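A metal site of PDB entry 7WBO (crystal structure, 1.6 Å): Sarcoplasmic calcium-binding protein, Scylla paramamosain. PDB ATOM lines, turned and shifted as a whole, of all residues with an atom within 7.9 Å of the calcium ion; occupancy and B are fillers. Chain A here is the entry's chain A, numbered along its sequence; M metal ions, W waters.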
ATOM      1  N   TYR A  27     -15.097  -0.020 -10.786  1.00  0.00           N
ATOM      2  CA  TYR A  27     -16.242   0.457 -11.601  1.00  0.00           C
ATOM      3  C   TYR A  27     -17.219  -0.671 -11.872  1.00  0.00           C
ATOM      4  O   TYR A  27     -16.895  -1.847 -11.644  1.00  0.00           O
ATOM      5  CB  TYR A  27     -15.781   1.056 -12.929  1.00  0.00           C
ATOM      6  CG  TYR A  27     -15.002   0.123 -13.836  1.00  0.00           C
ATOM      7  CD1 TYR A  27     -15.662  -0.740 -14.678  1.00  0.00           C
ATOM      8  CD2 TYR A  27     -13.619   0.016 -13.737  1.00  0.00           C
ATOM      9  CE1 TYR A  27     -14.985  -1.681 -15.452  1.00  0.00           C
ATOM     10  CE2 TYR A  27     -12.933  -0.882 -14.555  1.00  0.00           C
ATOM     11  CZ  TYR A  27     -13.615  -1.722 -15.395  1.00  0.00           C
ATOM     12  OH  TYR A  27     -12.962  -2.636 -16.191  1.00  0.00           O
ATOM     13  N   LEU A  28     -18.402  -0.361 -12.371  1.00  0.00           N
ATOM     14  CA  LEU A  28     -19.455  -1.368 -12.639  1.00  0.00           C
ATOM     15  C   LEU A  28     -19.480  -1.675 -14.134  1.00  0.00           C
ATOM     16  O   LEU A  28     -19.401  -0.726 -14.959  1.00  0.00           O
ATOM     17  CB  LEU A  28     -20.834  -0.864 -12.196  1.00  0.00           C
ATOM     18  CG  LEU A  28     -20.887  -0.423 -10.738  1.00  0.00           C
ATOM     19  CD1 LEU A  28     -22.288  -0.033 -10.350  1.00  0.00           C
ATOM     20  CD2 LEU A  28     -20.262  -1.458  -9.843  1.00  0.00           C
ATOM     21  N   TRP A  65     -28.428  -4.524 -14.642  1.00  0.00           N
ATOM     22  CA  TRP A  65     -27.287  -3.814 -15.282  1.00  0.00           C
ATOM     23  C   TRP A  65     -27.812  -2.938 -16.397  1.00  0.00           C
ATOM     24  O   TRP A  65     -27.371  -1.786 -16.500  1.00  0.00           O
ATOM     25  CB  TRP A  65     -26.262  -4.830 -15.756  1.00  0.00           C
ATOM     26  CG  TRP A  65     -25.215  -4.229 -16.627  1.00  0.00           C
ATOM     27  CD1 TRP A  65     -24.881  -4.653 -17.879  1.00  0.00           C
ATOM     28  CD2 TRP A  65     -24.433  -3.059 -16.384  1.00  0.00           C
ATOM     29  NE1 TRP A  65     -23.925  -3.845 -18.397  1.00  0.00           N
ATOM     30  CE2 TRP A  65     -23.606  -2.875 -17.506  1.00  0.00           C
ATOM     31  CE3 TRP A  65     -24.311  -2.156 -15.336  1.00  0.00           C
ATOM     32  CZ2 TRP A  65     -22.700  -1.819 -17.606  1.00  0.00           C
ATOM     33  CZ3 TRP A  65     -23.410  -1.132 -15.421  1.00  0.00           C
ATOM     34  CH2 TRP A  65     -22.656  -0.933 -16.567  1.00  0.00           C
ATOM     35  N   ALA A  69     -27.100   1.057 -16.299  1.00  0.00           N
ATOM     36  CA  ALA A  69     -26.352   1.723 -17.401  1.00  0.00           C
ATOM     37  C   ALA A  69     -27.277   2.754 -18.073  1.00  0.00           C
ATOM     38  O   ALA A  69     -26.764   3.851 -18.421  1.00  0.00           O
ATOM     39  CB  ALA A  69     -25.868   0.709 -18.382  1.00  0.00           C
ATOM     40  N   ALA A  72     -27.210   5.822 -15.700  1.00  0.00           N
ATOM     41  CA  ALA A  72     -25.953   6.303 -15.084  1.00  0.00           C
ATOM     42  C   ALA A  72     -24.748   6.325 -16.011  1.00  0.00           C
ATOM     43  O   ALA A  72     -23.739   6.891 -15.607  1.00  0.00           O
ATOM     44  CB  ALA A  72     -25.639   5.519 -13.822  1.00  0.00           C
ATOM     45  N   ASP A  73     -24.826   5.769 -17.228  1.00  0.00           N
ATOM     46  CA  ASP A  73     -23.636   5.729 -18.101  1.00  0.00           C
ATOM     47  C   ASP A  73     -23.523   7.042 -18.891  1.00  0.00           C
ATOM     48  O   ASP A  73     -23.687   7.074 -20.127  1.00  0.00           O
ATOM     49  CB  ASP A  73     -23.634   4.497 -19.001  1.00  0.00           C
ATOM     50  CG  ASP A  73     -22.322   4.349 -19.743  1.00  0.00           C
ATOM     51  OD1 ASP A  73     -21.323   5.042 -19.399  1.00  0.00           O
ATOM     52  OD2 ASP A  73     -22.343   3.507 -20.661  1.00  0.00           O
ATOM     53  N   PHE A  74     -23.133   8.098 -18.212  1.00  0.00           N
ATOM     54  CA  PHE A  74     -23.078   9.475 -18.740  1.00  0.00           C
ATOM     55  C   PHE A  74     -22.134   9.614 -19.926  1.00  0.00           C
ATOM     56  O   PHE A  74     -22.356  10.508 -20.737  1.00  0.00           O
ATOM     57  CB  PHE A  74     -22.720  10.479 -17.634  1.00  0.00           C
ATOM     58  CG  PHE A  74     -23.895  10.681 -16.683  1.00  0.00           C
ATOM     59  CD1 PHE A  74     -24.897  11.612 -16.958  1.00  0.00           C
ATOM     60  CD2 PHE A  74     -24.010   9.940 -15.511  1.00  0.00           C
ATOM     61  CE1 PHE A  74     -25.980  11.771 -16.115  1.00  0.00           C
ATOM     62  CE2 PHE A  74     -25.107  10.099 -14.667  1.00  0.00           C
ATOM     63  CZ  PHE A  74     -26.098  11.021 -14.994  1.00  0.00           C
ATOM     64  N   ASN A  75     -21.060   8.842 -19.976  1.00  0.00           N
ATOM     65  CA  ASN A  75     -20.111   8.956 -21.117  1.00  0.00           C
ATOM     66  C   ASN A  75     -20.291   7.802 -22.120  1.00  0.00           C
ATOM     67  O   ASN A  75     -19.431   7.687 -23.068  1.00  0.00           O
ATOM     68  CB  ASN A  75     -18.676   9.073 -20.651  1.00  0.00           C
ATOM     69  CG  ASN A  75     -18.085   7.761 -20.188  1.00  0.00           C
ATOM     70  OD1 ASN A  75     -18.832   6.871 -19.745  1.00  0.00           O
ATOM     71  ND2 ASN A  75     -16.769   7.644 -20.201  1.00  0.00           N
ATOM     72  N   LYS A  76     -21.351   7.020 -21.962  1.00  0.00           N
ATOM     73  CA  LYS A  76     -21.798   6.001 -22.954  1.00  0.00           C
ATOM     74  C   LYS A  76     -20.661   5.023 -23.266  1.00  0.00           C
ATOM     75  O   LYS A  76     -20.499   4.629 -24.443  1.00  0.00           O
ATOM     76  CB  LYS A  76     -22.231   6.718 -24.221  1.00  0.00           C
ATOM     77  CG  LYS A  76     -23.297   7.777 -23.964  1.00  0.00           C
ATOM     78  CD  LYS A  76     -23.908   8.193 -25.276  1.00  0.00           C
ATOM     79  CE  LYS A  76     -24.552   9.555 -25.192  1.00  0.00           C
ATOM     80  NZ  LYS A  76     -24.296  10.329 -26.434  1.00  0.00           N
ATOM     81  N   ASP A  77     -19.859   4.611 -22.292  1.00  0.00           N
ATOM     82  CA  ASP A  77     -18.704   3.720 -22.524  1.00  0.00           C
ATOM     83  C   ASP A  77     -18.933   2.285 -22.057  1.00  0.00           C
ATOM     84  O   ASP A  77     -17.972   1.500 -22.115  1.00  0.00           O
ATOM     85  CB  ASP A  77     -17.414   4.251 -21.923  1.00  0.00           C
ATOM     86  CG  ASP A  77     -17.327   4.285 -20.402  1.00  0.00           C
ATOM     87  OD1 ASP A  77     -18.322   3.992 -19.783  1.00  0.00           O
ATOM     88  OD2 ASP A  77     -16.216   4.662 -19.882  1.00  0.00           O
ATOM     89  N   GLY A  78     -20.117   1.934 -21.530  1.00  0.00           N
ATOM     90  CA  GLY A  78     -20.423   0.565 -21.110  1.00  0.00           C
ATOM     91  C   GLY A  78     -19.937   0.238 -19.722  1.00  0.00           C
ATOM     92  O   GLY A  78     -20.001  -0.929 -19.294  1.00  0.00           O
ATOM     93  N   GLN A  79     -19.505   1.254 -18.983  1.00  0.00           N
ATOM     94  CA  GLN A  79     -19.088   1.128 -17.575  1.00  0.00           C
ATOM     95  C   GLN A  79     -19.760   2.216 -16.771  1.00  0.00           C
ATOM     96  O   GLN A  79     -20.002   3.325 -17.305  1.00  0.00           O
ATOM     97  CB  GLN A  79     -17.584   1.258 -17.375  1.00  0.00           C
ATOM     98  CG  GLN A  79     -16.767   0.275 -18.194  1.00  0.00           C
ATOM     99  CD  GLN A  79     -15.264   0.461 -18.143  1.00  0.00           C
ATOM    100  OE1 GLN A  79     -14.713   1.465 -17.683  1.00  0.00           O
ATOM    101  NE2 GLN A  79     -14.582  -0.563 -18.645  1.00  0.00           N
ATOM    102  N   VAL A  80     -20.011   1.931 -15.507  1.00  0.00           N
ATOM    103  CA  VAL A  80     -20.548   3.003 -14.627  1.00  0.00           C
ATOM    104  C   VAL A  80     -19.563   3.223 -13.490  1.00  0.00           C
ATOM    105  O   VAL A  80     -19.291   2.290 -12.687  1.00  0.00           O
ATOM    106  CB  VAL A  80     -21.961   2.665 -14.102  1.00  0.00           C
ATOM    107  CG1 VAL A  80     -22.400   3.566 -12.969  1.00  0.00           C
ATOM    108  CG2 VAL A  80     -22.974   2.720 -15.201  1.00  0.00           C
ATOM    109  N   THR A  81     -19.025   4.435 -13.417  1.00  0.00           N
ATOM    110  CA  THR A  81     -18.033   4.785 -12.387  1.00  0.00           C
ATOM    111  C   THR A  81     -18.758   5.170 -11.089  1.00  0.00           C
ATOM    112  O   THR A  81     -20.002   5.403 -11.092  1.00  0.00           O
ATOM    113  CB  THR A  81     -17.144   5.938 -12.810  1.00  0.00           C
ATOM    114  OG1 THR A  81     -18.018   7.074 -13.003  1.00  0.00           O
ATOM    115  CG2 THR A  81     -16.435   5.633 -14.102  1.00  0.00           C
ATOM    116  N   GLU A  84     -20.366   8.549 -11.791  1.00  0.00           N
ATOM    117  CA  GLU A  84     -21.606   8.367 -12.573  1.00  0.00           C
ATOM    118  C   GLU A  84     -22.754   7.860 -11.686  1.00  0.00           C
ATOM    119  O   GLU A  84     -23.890   8.400 -11.787  1.00  0.00           O
ATOM    120  CB  GLU A  84     -21.341   7.443 -13.760  1.00  0.00           C
ATOM    121  CG  GLU A  84     -20.531   8.053 -14.907  1.00  0.00           C
ATOM    122  CD  GLU A  84     -20.212   7.086 -16.044  1.00  0.00           C
ATOM    123  OE1 GLU A  84     -19.949   5.927 -15.786  1.00  0.00           O
ATOM    124  OE2 GLU A  84     -20.237   7.556 -17.221  1.00  0.00           O
HETATM  125 CA    CA M   1     -19.449   5.383 -18.115  1.00  0.00          CA
HETATM  126  O   HOH W   1     -17.191   5.588 -17.381  1.00  0.00           O
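The side-chain carboxylate (OD1) of Asp 73 sits close to the backbone NH (N) of Lys 76 (3.2 Å). The backbone NH (N) of Gly 78 lies within hydrogen-bond range of the side-chain carboxylate (OD2) of Asp 73 (2.9 Å). The side-chain carboxylate of Glu 84 lies close to the backbone NH of Phe 74 (3.1 Å). The backbone NH (N) of Glu 84 sits at hydrogen-bond distance from the side-chain hydroxyl (OG1) of Thr 81, at 3.0 Å.
O of Gln 79 binds the calcium ion, 2.3 Å away. The side-chain amide oxygen (OD1) of Asn 75 is bound to the calcium ion, at 2.3 Å. The side-chain carboxylate (OD1) of Asp 73 is bound to the calcium ion, 2.3 Å away. Water W1 binds the calcium ion, 2.4 Å away. OE1 of Glu 84 binds the calcium ion. The calcium ion is bound by OD1 of Asp 77 (2.4 Å). The side-chain carboxylate (OE2) of Glu 84 is bound to the calcium ion, 2.5 Å away.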
